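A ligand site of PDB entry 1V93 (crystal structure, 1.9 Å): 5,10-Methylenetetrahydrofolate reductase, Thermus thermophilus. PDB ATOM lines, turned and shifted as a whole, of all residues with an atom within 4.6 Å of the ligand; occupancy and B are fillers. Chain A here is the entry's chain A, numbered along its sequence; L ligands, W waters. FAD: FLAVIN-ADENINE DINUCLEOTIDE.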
ATOM      1  N   GLU A  18     -30.152  13.949  26.192  1.00  0.00           N
ATOM      2  CA  GLU A  18     -29.960  15.255  25.577  1.00  0.00           C
ATOM      3  C   GLU A  18     -30.783  16.335  26.254  1.00  0.00           C
ATOM      4  O   GLU A  18     -31.878  16.080  26.736  1.00  0.00           O
ATOM      5  CB  GLU A  18     -30.359  15.157  24.107  1.00  0.00           C
ATOM      6  CG  GLU A  18     -30.088  16.380  23.276  1.00  0.00           C
ATOM      7  CD  GLU A  18     -30.304  16.113  21.793  1.00  0.00           C
ATOM      8  OE1 GLU A  18     -29.918  15.019  21.327  1.00  0.00           O
ATOM      9  OE2 GLU A  18     -30.830  17.004  21.095  1.00  0.00           O
ATOM     10  N   THR A  49     -28.116  20.250  22.826  1.00  0.00           N
ATOM     11  CA  THR A  49     -28.740  20.647  21.579  1.00  0.00           C
ATOM     12  C   THR A  49     -28.263  22.034  21.176  1.00  0.00           C
ATOM     13  O   THR A  49     -28.020  22.875  22.024  1.00  0.00           O
ATOM     14  CB  THR A  49     -30.275  20.659  21.719  1.00  0.00           C
ATOM     15  OG1 THR A  49     -30.707  19.419  22.281  1.00  0.00           O
ATOM     16  CG2 THR A  49     -30.947  20.838  20.366  1.00  0.00           C
ATOM     17  N   TYR A  50     -28.122  22.248  19.870  1.00  0.00           N
ATOM     18  CA  TYR A  50     -27.655  23.532  19.355  1.00  0.00           C
ATOM     19  C   TYR A  50     -28.831  24.307  18.791  1.00  0.00           C
ATOM     20  O   TYR A  50     -29.512  23.854  17.858  1.00  0.00           O
ATOM     21  CB  TYR A  50     -26.611  23.284  18.261  1.00  0.00           C
ATOM     22  CG  TYR A  50     -25.798  24.492  17.828  1.00  0.00           C
ATOM     23  CD1 TYR A  50     -24.855  25.057  18.684  1.00  0.00           C
ATOM     24  CD2 TYR A  50     -25.971  25.059  16.567  1.00  0.00           C
ATOM     25  CE1 TYR A  50     -24.087  26.148  18.278  1.00  0.00           C
ATOM     26  CE2 TYR A  50     -25.210  26.159  16.155  1.00  0.00           C
ATOM     27  CZ  TYR A  50     -24.272  26.695  17.018  1.00  0.00           C
ATOM     28  OH  TYR A  50     -23.502  27.768  16.614  1.00  0.00           O
ATOM     29  N   ALA A  52     -31.346  26.640  16.813  1.00  0.00           N
ATOM     30  CA  ALA A  52     -31.471  26.814  15.375  1.00  0.00           C
ATOM     31  C   ALA A  52     -30.599  27.938  14.816  1.00  0.00           C
ATOM     32  O   ALA A  52     -30.633  29.076  15.293  1.00  0.00           O
ATOM     33  CB  ALA A  52     -32.925  27.053  15.012  1.00  0.00           C
ATOM     34  N   HIS A  77     -23.525  19.666  20.282  1.00  0.00           N
ATOM     35  CA  HIS A  77     -24.135  19.662  18.955  1.00  0.00           C
ATOM     36  C   HIS A  77     -23.716  20.954  18.262  1.00  0.00           C
ATOM     37  O   HIS A  77     -23.528  21.987  18.920  1.00  0.00           O
ATOM     38  CB  HIS A  77     -25.664  19.637  19.075  1.00  0.00           C
ATOM     39  CG  HIS A  77     -26.224  18.323  19.530  1.00  0.00           C
ATOM     40  ND1 HIS A  77     -25.516  17.424  20.291  1.00  0.00           N
ATOM     41  CD2 HIS A  77     -27.465  17.784  19.360  1.00  0.00           C
ATOM     42  CE1 HIS A  77     -26.290  16.388  20.578  1.00  0.00           C
ATOM     43  NE2 HIS A  77     -27.471  16.578  20.017  1.00  0.00           N
ATOM     44  N   THR A  79     -24.464  22.890  14.278  1.00  0.00           N
ATOM     45  CA  THR A  79     -25.043  22.869  12.930  1.00  0.00           C
ATOM     46  C   THR A  79     -24.337  23.909  12.077  1.00  0.00           C
ATOM     47  O   THR A  79     -23.606  24.744  12.613  1.00  0.00           O
ATOM     48  CB  THR A  79     -26.558  23.204  12.971  1.00  0.00           C
ATOM     49  OG1 THR A  79     -26.737  24.567  13.399  1.00  0.00           O
ATOM     50  CG2 THR A  79     -27.284  22.282  13.933  1.00  0.00           C
ATOM     51  N   LEU A 104     -21.257  16.591  17.819  1.00  0.00           N
ATOM     52  CA  LEU A 104     -22.267  15.984  16.964  1.00  0.00           C
ATOM     53  C   LEU A 104     -22.393  16.967  15.813  1.00  0.00           C
ATOM     54  O   LEU A 104     -22.966  18.048  15.967  1.00  0.00           O
ATOM     55  CB  LEU A 104     -23.606  15.814  17.687  1.00  0.00           C
ATOM     56  CG  LEU A 104     -24.544  14.814  16.995  1.00  0.00           C
ATOM     57  CD1 LEU A 104     -23.970  13.394  17.124  1.00  0.00           C
ATOM     58  CD2 LEU A 104     -25.931  14.865  17.598  1.00  0.00           C
ATOM     59  N   ALA A 105     -21.813  16.622  14.670  1.00  0.00           N
ATOM     60  CA  ALA A 105     -21.831  17.479  13.496  1.00  0.00           C
ATOM     61  C   ALA A 105     -23.144  17.355  12.744  1.00  0.00           C
ATOM     62  O   ALA A 105     -23.494  16.281  12.270  1.00  0.00           O
ATOM     63  CB  ALA A 105     -20.648  17.120  12.569  1.00  0.00           C
ATOM     64  N   LEU A 106     -23.864  18.476  12.636  1.00  0.00           N
ATOM     65  CA  LEU A 106     -25.173  18.520  11.997  1.00  0.00           C
ATOM     66  C   LEU A 106     -25.316  19.646  10.980  1.00  0.00           C
ATOM     67  O   LEU A 106     -24.558  20.614  11.009  1.00  0.00           O
ATOM     68  CB  LEU A 106     -26.238  18.720  13.054  1.00  0.00           C
ATOM     69  CG  LEU A 106     -26.266  17.715  14.205  1.00  0.00           C
ATOM     70  CD1 LEU A 106     -26.556  18.433  15.513  1.00  0.00           C
ATOM     71  CD2 LEU A 106     -27.273  16.627  13.898  1.00  0.00           C
ATOM     72  N   ARG A 107     -26.317  19.529  10.105  1.00  0.00           N
ATOM     73  CA  ARG A 107     -26.568  20.585   9.131  1.00  0.00           C
ATOM     74  C   ARG A 107     -27.543  21.602   9.718  1.00  0.00           C
ATOM     75  O   ARG A 107     -27.312  22.809   9.628  1.00  0.00           O
ATOM     76  CB  ARG A 107     -27.188  20.019   7.853  1.00  0.00           C
ATOM     77  CG  ARG A 107     -27.408  21.101   6.779  1.00  0.00           C
ATOM     78  CD  ARG A 107     -28.414  20.685   5.720  1.00  0.00           C
ATOM     79  NE  ARG A 107     -29.771  20.582   6.240  1.00  0.00           N
ATOM     80  CZ  ARG A 107     -30.832  20.238   5.516  1.00  0.00           C
ATOM     81  NH1 ARG A 107     -30.693  19.961   4.219  1.00  0.00           N
ATOM     82  NH2 ARG A 107     -32.031  20.158   6.082  1.00  0.00           N
ATOM     83  N   GLY A 108     -28.611  21.109  10.333  1.00  0.00           N
ATOM     84  CA  GLY A 108     -29.612  21.991  10.893  1.00  0.00           C
ATOM     85  C   GLY A 108     -30.757  22.078   9.902  1.00  0.00           C
ATOM     86  O   GLY A 108     -30.569  21.814   8.714  1.00  0.00           O
ATOM     87  N   ASP A 109     -31.950  22.431  10.371  1.00  0.00           N
ATOM     88  CA  ASP A 109     -33.100  22.512   9.479  1.00  0.00           C
ATOM     89  C   ASP A 109     -33.184  23.816   8.705  1.00  0.00           C
ATOM     90  O   ASP A 109     -32.420  24.739   8.970  1.00  0.00           O
ATOM     91  CB  ASP A 109     -34.393  22.285  10.262  1.00  0.00           C
ATOM     92  CG  ASP A 109     -34.565  20.839  10.676  1.00  0.00           C
ATOM     93  OD1 ASP A 109     -34.732  19.983   9.785  1.00  0.00           O
ATOM     94  OD2 ASP A 109     -34.522  20.556  11.887  1.00  0.00           O
ATOM     95  N   TYR A 126     -23.859  20.856   3.809  1.00  0.00           N
ATOM     96  CA  TYR A 126     -24.069  19.505   4.321  1.00  0.00           C
ATOM     97  C   TYR A 126     -23.290  19.240   5.605  1.00  0.00           C
ATOM     98  O   TYR A 126     -22.193  19.775   5.807  1.00  0.00           O
ATOM     99  CB  TYR A 126     -23.651  18.476   3.277  1.00  0.00           C
ATOM    100  CG  TYR A 126     -24.330  18.644   1.929  1.00  0.00           C
ATOM    101  CD1 TYR A 126     -25.711  18.504   1.805  1.00  0.00           C
ATOM    102  CD2 TYR A 126     -23.588  18.943   0.791  1.00  0.00           C
ATOM    103  CE1 TYR A 126     -26.338  18.668   0.568  1.00  0.00           C
ATOM    104  CE2 TYR A 126     -24.199  19.096  -0.452  1.00  0.00           C
ATOM    105  CZ  TYR A 126     -25.575  18.954  -0.555  1.00  0.00           C
ATOM    106  OH  TYR A 126     -26.190  19.074  -1.782  1.00  0.00           O
ATOM    107  N   ALA A 127     -23.848  18.394   6.470  1.00  0.00           N
ATOM    108  CA  ALA A 127     -23.193  18.042   7.719  1.00  0.00           C
ATOM    109  C   ALA A 127     -21.825  17.423   7.458  1.00  0.00           C
ATOM    110  O   ALA A 127     -20.891  17.609   8.234  1.00  0.00           O
ATOM    111  CB  ALA A 127     -24.061  17.077   8.511  1.00  0.00           C
ATOM    112  N   ALA A 147     -26.155  12.481  12.648  1.00  0.00           N
ATOM    113  CA  ALA A 147     -27.538  12.023  12.693  1.00  0.00           C
ATOM    114  C   ALA A 147     -27.845  10.975  11.642  1.00  0.00           C
ATOM    115  O   ALA A 147     -27.348  11.034  10.524  1.00  0.00           O
ATOM    116  CB  ALA A 147     -28.476  13.217  12.512  1.00  0.00           C
ATOM    117  N   ALA A 148     -28.666   9.987  12.024  1.00  0.00           N
ATOM    118  CA  ALA A 148     -29.086   8.911  11.129  1.00  0.00           C
ATOM    119  C   ALA A 148     -30.606   8.925  11.134  1.00  0.00           C
ATOM    120  O   ALA A 148     -31.212   9.241  12.159  1.00  0.00           O
ATOM    121  CB  ALA A 148     -28.562   7.567  11.629  1.00  0.00           C
ATOM    122  N   TYR A 149     -31.222   8.560  10.010  1.00  0.00           N
ATOM    123  CA  TYR A 149     -32.676   8.554   9.890  1.00  0.00           C
ATOM    124  C   TYR A 149     -33.279   7.226   9.474  1.00  0.00           C
ATOM    125  O   TYR A 149     -33.353   6.898   8.275  1.00  0.00           O
ATOM    126  CB  TYR A 149     -33.120   9.668   8.936  1.00  0.00           C
ATOM    127  CG  TYR A 149     -32.591  11.022   9.344  1.00  0.00           C
ATOM    128  CD1 TYR A 149     -31.319  11.441   8.937  1.00  0.00           C
ATOM    129  CD2 TYR A 149     -33.317  11.848  10.202  1.00  0.00           C
ATOM    130  CE1 TYR A 149     -30.781  12.641   9.376  1.00  0.00           C
ATOM    131  CE2 TYR A 149     -32.787  13.050  10.652  1.00  0.00           C
ATOM    132  CZ  TYR A 149     -31.520  13.444  10.244  1.00  0.00           C
ATOM    133  OH  TYR A 149     -31.002  14.632  10.687  1.00  0.00           O
ATOM    134  N   HIS A 153     -34.637  10.991   5.943  1.00  0.00           N
ATOM    135  CA  HIS A 153     -34.715  12.416   6.223  1.00  0.00           C
ATOM    136  C   HIS A 153     -35.776  12.983   5.296  1.00  0.00           C
ATOM    137  O   HIS A 153     -35.840  12.618   4.123  1.00  0.00           O
ATOM    138  CB  HIS A 153     -33.360  13.097   5.968  1.00  0.00           C
ATOM    139  CG  HIS A 153     -33.357  14.566   6.247  1.00  0.00           C
ATOM    140  ND1 HIS A 153     -33.919  15.479   5.380  1.00  0.00           N
ATOM    141  CD2 HIS A 153     -32.948  15.266   7.326  1.00  0.00           C
ATOM    142  CE1 HIS A 153     -33.852  16.695   5.920  1.00  0.00           C
ATOM    143  NE2 HIS A 153     -33.271  16.589   7.098  1.00  0.00           N
ATOM    144  N   GLU A 155     -36.125  15.543   3.518  1.00  0.00           N
ATOM    145  CA  GLU A 155     -35.675  16.142   2.271  1.00  0.00           C
ATOM    146  C   GLU A 155     -35.026  15.185   1.275  1.00  0.00           C
ATOM    147  O   GLU A 155     -34.800  15.568   0.129  1.00  0.00           O
ATOM    148  CB  GLU A 155     -34.719  17.301   2.583  1.00  0.00           C
ATOM    149  CG  GLU A 155     -35.383  18.500   3.232  1.00  0.00           C
ATOM    150  CD  GLU A 155     -34.373  19.487   3.803  1.00  0.00           C
ATOM    151  OE1 GLU A 155     -33.401  19.812   3.098  1.00  0.00           O
ATOM    152  OE2 GLU A 155     -34.551  19.929   4.962  1.00  0.00           O
ATOM    153  N   SER A 156     -34.718  13.960   1.693  1.00  0.00           N
ATOM    154  CA  SER A 156     -34.088  13.000   0.787  1.00  0.00           C
ATOM    155  C   SER A 156     -35.015  12.632  -0.383  1.00  0.00           C
ATOM    156  O   SER A 156     -36.217  12.456  -0.198  1.00  0.00           O
ATOM    157  CB  SER A 156     -33.688  11.735   1.557  1.00  0.00           C
ATOM    158  OG  SER A 156     -32.653  12.021   2.489  1.00  0.00           O
ATOM    159  N   ALA A 161     -31.007   7.186  -1.725  1.00  0.00           N
ATOM    160  CA  ALA A 161     -30.200   8.406  -1.686  1.00  0.00           C
ATOM    161  C   ALA A 161     -29.896   8.789  -0.244  1.00  0.00           C
ATOM    162  O   ALA A 161     -28.781   9.162   0.098  1.00  0.00           O
ATOM    163  CB  ALA A 161     -30.919   9.548  -2.374  1.00  0.00           C
ATOM    164  N   ASP A 162     -30.915   8.688   0.604  1.00  0.00           N
ATOM    165  CA  ASP A 162     -30.760   9.016   2.018  1.00  0.00           C
ATOM    166  C   ASP A 162     -29.624   8.191   2.635  1.00  0.00           C
ATOM    167  O   ASP A 162     -28.804   8.701   3.394  1.00  0.00           O
ATOM    168  CB  ASP A 162     -32.066   8.731   2.770  1.00  0.00           C
ATOM    169  CG  ASP A 162     -32.035   9.197   4.213  1.00  0.00           C
ATOM    170  OD1 ASP A 162     -32.074  10.427   4.444  1.00  0.00           O
ATOM    171  OD2 ASP A 162     -31.952   8.337   5.123  1.00  0.00           O
ATOM    172  N   HIS A 165     -26.079   9.185   1.196  1.00  0.00           N
ATOM    173  CA  HIS A 165     -25.619  10.417   1.811  1.00  0.00           C
ATOM    174  C   HIS A 165     -25.152  10.190   3.242  1.00  0.00           C
ATOM    175  O   HIS A 165     -24.201  10.822   3.691  1.00  0.00           O
ATOM    176  CB  HIS A 165     -26.745  11.449   1.760  1.00  0.00           C
ATOM    177  CG  HIS A 165     -27.201  11.746   0.367  1.00  0.00           C
ATOM    178  ND1 HIS A 165     -28.409  12.359   0.079  1.00  0.00           N
ATOM    179  CD2 HIS A 165     -26.608  11.506  -0.833  1.00  0.00           C
ATOM    180  CE1 HIS A 165     -28.536  12.480  -1.229  1.00  0.00           C
ATOM    181  NE2 HIS A 165     -27.463  11.972  -1.804  1.00  0.00           N
ATOM    182  N   LYS A 169     -21.417  10.722   4.722  1.00  0.00           N
ATOM    183  CA  LYS A 169     -21.165  11.487   5.939  1.00  0.00           C
ATOM    184  C   LYS A 169     -20.284  10.669   6.879  1.00  0.00           C
ATOM    185  O   LYS A 169     -19.383  11.209   7.529  1.00  0.00           O
ATOM    186  CB  LYS A 169     -22.493  11.858   6.624  1.00  0.00           C
ATOM    187  CG  LYS A 169     -22.338  12.613   7.938  1.00  0.00           C
ATOM    188  CD  LYS A 169     -23.626  13.326   8.375  1.00  0.00           C
ATOM    189  CE  LYS A 169     -24.783  12.364   8.590  1.00  0.00           C
ATOM    190  NZ  LYS A 169     -26.043  13.115   8.934  1.00  0.00           N
ATOM    191  N   ILE A 178     -26.284   8.805  15.962  1.00  0.00           N
ATOM    192  CA  ILE A 178     -27.449   8.715  16.840  1.00  0.00           C
ATOM    193  C   ILE A 178     -28.647   8.857  15.912  1.00  0.00           C
ATOM    194  O   ILE A 178     -28.671   9.736  15.057  1.00  0.00           O
ATOM    195  CB  ILE A 178     -27.479   9.849  17.882  1.00  0.00           C
ATOM    196  CG1 ILE A 178     -26.209   9.794  18.743  1.00  0.00           C
ATOM    197  CG2 ILE A 178     -28.718   9.722  18.764  1.00  0.00           C
ATOM    198  CD1 ILE A 178     -26.155  10.861  19.828  1.00  0.00           C
ATOM    199  N   THR A 179     -29.647   7.991  16.065  1.00  0.00           N
ATOM    200  CA  THR A 179     -30.797   8.068  15.182  1.00  0.00           C
ATOM    201  C   THR A 179     -31.866   9.035  15.641  1.00  0.00           C
ATOM    202  O   THR A 179     -31.972   9.384  16.828  1.00  0.00           O
ATOM    203  CB  THR A 179     -31.501   6.705  14.998  1.00  0.00           C
ATOM    204  OG1 THR A 179     -32.369   6.455  16.117  1.00  0.00           O
ATOM    205  CG2 THR A 179     -30.482   5.571  14.881  1.00  0.00           C
ATOM    206  N   GLN A 180     -32.665   9.454  14.667  1.00  0.00           N
ATOM    207  CA  GLN A 180     -33.816  10.313  14.898  1.00  0.00           C
ATOM    208  C   GLN A 180     -34.697   9.421  15.763  1.00  0.00           C
ATOM    209  O   GLN A 180     -34.521   8.193  15.759  1.00  0.00           O
ATOM    210  CB  GLN A 180     -34.509  10.604  13.559  1.00  0.00           C
ATOM    211  CG  GLN A 180     -35.803  11.407  13.647  1.00  0.00           C
ATOM    212  CD  GLN A 180     -35.622  12.700  14.421  1.00  0.00           C
ATOM    213  OE1 GLN A 180     -35.577  12.702  15.660  1.00  0.00           O
ATOM    214  NE2 GLN A 180     -35.494  13.805  13.698  1.00  0.00           N
ATOM    215  N   TYR A 272     -34.111  11.605  24.499  1.00  0.00           N
ATOM    216  CA  TYR A 272     -34.481  12.989  24.235  1.00  0.00           C
ATOM    217  C   TYR A 272     -35.407  13.353  25.402  1.00  0.00           C
ATOM    218  O   TYR A 272     -36.558  12.915  25.457  1.00  0.00           O
ATOM    219  CB  TYR A 272     -35.233  13.103  22.893  1.00  0.00           C
ATOM    220  CG  TYR A 272     -34.406  12.689  21.688  1.00  0.00           C
ATOM    221  CD1 TYR A 272     -34.742  11.559  20.946  1.00  0.00           C
ATOM    222  CD2 TYR A 272     -33.294  13.443  21.293  1.00  0.00           C
ATOM    223  CE1 TYR A 272     -33.988  11.177  19.827  1.00  0.00           C
ATOM    224  CE2 TYR A 272     -32.527  13.075  20.182  1.00  0.00           C
ATOM    225  CZ  TYR A 272     -32.886  11.944  19.450  1.00  0.00           C
ATOM    226  OH  TYR A 272     -32.129  11.594  18.349  1.00  0.00           O
HETATM  227  PA  FAD L   1     -27.287  16.003   6.430  1.00  0.00           P
HETATM  228  O1A FAD L   1     -26.739  14.667   6.741  1.00  0.00           O
HETATM  229  O2A FAD L   1     -26.372  17.026   5.828  1.00  0.00           O
HETATM  230  O5B FAD L   1     -28.565  15.781   5.511  1.00  0.00           O
HETATM  231  C5B FAD L   1     -29.402  16.864   5.020  1.00  0.00           C
HETATM  232  C4B FAD L   1     -30.113  16.420   3.718  1.00  0.00           C
HETATM  233  O4B FAD L   1     -29.114  16.547   2.667  1.00  0.00           O
HETATM  234  C3B FAD L   1     -30.621  14.955   3.670  1.00  0.00           C
HETATM  235  O3B FAD L   1     -31.894  14.839   3.081  1.00  0.00           O
HETATM  236  C2B FAD L   1     -29.529  14.249   2.898  1.00  0.00           C
HETATM  237  O2B FAD L   1     -29.903  13.029   2.254  1.00  0.00           O
HETATM  238  C1B FAD L   1     -29.028  15.324   1.940  1.00  0.00           C
HETATM  239  N9A FAD L   1     -27.632  15.226   1.516  1.00  0.00           N
HETATM  240  C8A FAD L   1     -26.531  14.945   2.301  1.00  0.00           C
HETATM  241  N7A FAD L   1     -25.402  14.933   1.618  1.00  0.00           N
HETATM  242  C5A FAD L   1     -25.776  15.222   0.322  1.00  0.00           C
HETATM  243  C6A FAD L   1     -25.047  15.358  -0.893  1.00  0.00           C
HETATM  244  N6A FAD L   1     -23.709  15.208  -0.935  1.00  0.00           N
HETATM  245  N1A FAD L   1     -25.724  15.652  -2.025  1.00  0.00           N
HETATM  246  C2A FAD L   1     -27.097  15.804  -1.981  1.00  0.00           C
HETATM  247  N3A FAD L   1     -27.880  15.694  -0.888  1.00  0.00           N
HETATM  248  C4A FAD L   1     -27.147  15.396   0.264  1.00  0.00           C
HETATM  249  N1  FAD L   1     -30.982  20.233  14.645  1.00  0.00           N
HETATM  250  C2  FAD L   1     -30.569  21.388  15.242  1.00  0.00           C
HETATM  251  O2  FAD L   1     -30.851  22.533  14.770  1.00  0.00           O
HETATM  252  N3  FAD L   1     -29.833  21.358  16.425  1.00  0.00           N
HETATM  253  C4  FAD L   1     -29.433  20.169  17.055  1.00  0.00           C
HETATM  254  O4  FAD L   1     -28.777  20.215  18.121  1.00  0.00           O
HETATM  255  C4X FAD L   1     -29.845  18.962  16.419  1.00  0.00           C
HETATM  256  N5  FAD L   1     -29.473  17.728  16.991  1.00  0.00           N
HETATM  257  C5X FAD L   1     -29.898  16.569  16.369  1.00  0.00           C
HETATM  258  C6  FAD L   1     -29.538  15.321  16.933  1.00  0.00           C
HETATM  259  C7  FAD L   1     -29.925  14.114  16.365  1.00  0.00           C
HETATM  260  C7M FAD L   1     -29.474  12.820  17.051  1.00  0.00           C
HETATM  261  C8  FAD L   1     -30.728  14.102  15.182  1.00  0.00           C
HETATM  262  C8M FAD L   1     -31.203  12.843  14.507  1.00  0.00           C
HETATM  263  C9  FAD L   1     -31.096  15.360  14.612  1.00  0.00           C
HETATM  264  C9A FAD L   1     -30.710  16.594  15.160  1.00  0.00           C
HETATM  265  N10 FAD L   1     -31.058  17.861  14.595  1.00  0.00           N
HETATM  266  C10 FAD L   1     -30.618  19.075  15.224  1.00  0.00           C
HETATM  267  C1' FAD L   1     -31.876  18.000  13.369  1.00  0.00           C
HETATM  268  C2' FAD L   1     -31.111  18.057  12.055  1.00  0.00           C
HETATM  269  O2' FAD L   1     -30.223  19.202  12.075  1.00  0.00           O
HETATM  270  C3' FAD L   1     -32.121  18.101  10.892  1.00  0.00           C
HETATM  271  O3' FAD L   1     -32.686  16.797  10.773  1.00  0.00           O
HETATM  272  C4' FAD L   1     -31.498  18.534   9.565  1.00  0.00           C
HETATM  273  O4' FAD L   1     -32.561  18.867   8.649  1.00  0.00           O
HETATM  274  C5' FAD L   1     -30.583  17.491   8.965  1.00  0.00           C
HETATM  275  O5' FAD L   1     -29.295  17.491   9.639  1.00  0.00           O
HETATM  276  P   FAD L   1     -28.184  16.432   9.255  1.00  0.00           P
HETATM  277  O1P FAD L   1     -27.004  16.691  10.080  1.00  0.00           O
HETATM  278  O2P FAD L   1     -28.811  15.071   9.344  1.00  0.00           O
HETATM  279  O3P FAD L   1     -27.931  16.721   7.706  1.00  0.00           O
HETATM  280  O   HOH W   1     -35.332  16.396   9.970  1.00  0.00           O
HETATM  281  O   HOH W   2     -29.885  24.745  13.388  1.00  0.00           O
HETATM  282  O   HOH W   3     -22.584  16.587  -3.493  1.00  0.00           O
HETATM  283  O   HOH W   4     -23.485  13.545   3.051  1.00  0.00           O
HETATM  284  O   HOH W   5     -32.318  17.176  18.924  1.00  0.00           O
HETATM  285  O   HOH W   6     -29.211  10.882   4.842  1.00  0.00           O
HETATM  286  O   HOH W   7     -32.899  22.249  13.084  1.00  0.00           O
HETATM  287  O   HOH W   8     -32.390  23.036  17.843  1.00  0.00           O
HETATM  288  O   HOH W   9     -31.689  16.627   0.090  1.00  0.00           O
HETATM  289  O   HOH W  10     -21.531  14.438   1.329  1.00  0.00           O
HETATM  290  O   HOH W  11     -25.036  16.356  -4.558  1.00  0.00           O
HETATM  291  O   HOH W  12     -25.432  14.838  11.232  1.00  0.00           O
HETATM  292  O   HOH W  13     -23.845  15.250   5.289  1.00  0.00           O
HETATM  293  O   HOH W  14     -34.499  16.503  14.906  1.00  0.00           O
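A ring nitrogen (ND1) of His 165 lies close to the backbone carbonyl oxygen of Ala 161 (3.2 Å). O of Ala 147 lies within hydrogen-bond range of NZ of Lys 169, 2.9 Å away. The backbone NH (N) of Glu 155 sits at hydrogen-bond distance from a ring nitrogen (ND1) of His 153 (2.9 Å). The backbone NH of His 153 is in hydrogen-bond range of the side-chain carboxylate of Asp 162 (3.0 Å). NH2 of Arg 107 is in salt-bridge range of OE2 of Glu 155, 2.8 Å away. OG1 of Thr 49 lies within hydrogen-bond range of OE2 of Glu 18, at 2.7 Å. OH of Tyr 272 lies within hydrogen-bond range of O of Thr 179 (2.7 Å). The backbone NH of Ala 148 lies within hydrogen-bond range of the backbone carbonyl oxygen of Ile 178 (3.0 Å).
The side-chain hydroxyl of Tyr 149 is in hydrogen-bond range of an oxygen (O2P) of the ligand (2.6 Å). The side-chain carboxylate (OD1) of Asp 109 sits at hydrogen-bond distance from an oxygen (O4') of the ligand (2.7 Å). ND1 of His 165 lies within hydrogen-bond range of O2B of the ligand (2.7 Å). An oxygen (O4) of the ligand is in hydrogen-bond range of the backbone NH of Tyr 50 (2.8 Å). O of Tyr 50 lies within hydrogen-bond range of N3 of the ligand, at 2.9 Å. An oxygen (O1A) of the ligand lies within salt-bridge range of the side-chain amino group of Lys 169, at 2.8 Å. O4' of the ligand lies within hydrogen-bond range of NE2 of His 153 (2.8 Å). The backbone NH (N) of Arg 107 lies within hydrogen-bond range of an oxygen (O1P) of the ligand (2.9 Å). NH2 of Arg 107 is in hydrogen-bond range of O4' of the ligand (2.9 Å). O3B of the ligand is in hydrogen-bond range of N of Ser 156 (3.3 Å). An oxygen (O2B) of the ligand is in hydrogen-bond range of the side-chain hydroxyl (OG) of Ser 156 (2.9 Å). O2A of the ligand sits at hydrogen-bond distance from N of Ala 127 (2.9 Å). An oxygen (O2') of the ligand is in hydrogen-bond range of the backbone NH (N) of Gly 108. N1A of the ligand lies close to OH of Tyr 126 (3.5 Å).
Water W12 lies within hydrogen-bond range of the backbone carbonyl oxygen (O) of Ala 105 (2.6 Å), an oxygen (O1P) of the ligand (2.7 Å), the backbone NH (N) of Ala 147 (2.8 Å) and the side-chain amino group (NZ) of Lys 169 (2.9 Å). Water W4 bridges N7A of the ligand (2.8 Å) and O of His 165 (2.9 Å). Water W2 bridges O2 of the ligand (2.8 Å) and OG1 of Thr 79 (3.2 Å). Water W8 lies within hydrogen-bond range of O of Tyr 50 and N3 of the ligand. Water W6 lies within hydrogen-bond range of the backbone carbonyl oxygen of Asp 162 (2.6 Å) and an oxygen (O2B) of the ligand (3.4 Å). Water W9 lies within hydrogen-bond range of O of Glu 155 and O3B of the ligand.
CG2 of Thr 49 touches O4 of the ligand (3.2 Å). His 77 touches the ligand (CD2 to O4, 3.0 Å). Thr 79 touches the ligand (CG2 to C2, 3.6 Å). CD2 of Leu 104 touches C6 of the ligand (3.7 Å). CA of Leu 106 touches O1P of the ligand, 3.2 Å away. Ala 147 touches the ligand (CB to C8M, 3.4 Å). Glu 155 touches the ligand. Ile 178 touches the ligand (CG2 to C7M, 3.6 Å). Gln 180 touches the ligand (CA to C8M, 3.7 Å). Tyr 272 touches the ligand. Hydrophobic or aromatic side chains within 4 Å of the ligand: Tyr 50, His 77, Leu 104, Leu 106, Tyr 126, Ala 127, Ala 147, Tyr 149, His 153, His 165 and Ile 178. 21 residues have an atom within 4 Å of the ligand: Thr 49, Tyr 50, His 77, Thr 79, Leu 104, Leu 106, Arg 107, Gly 108, Asp 109, Tyr 126, Ala 127, Ala 147, Tyr 149, His 153, Glu 155, Ser 156, His 165, Lys 169, Ile 178, Gln 180 and Tyr 272. The nearest printed residue that does not touch the ligand is Thr 179 (4.03 Å).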
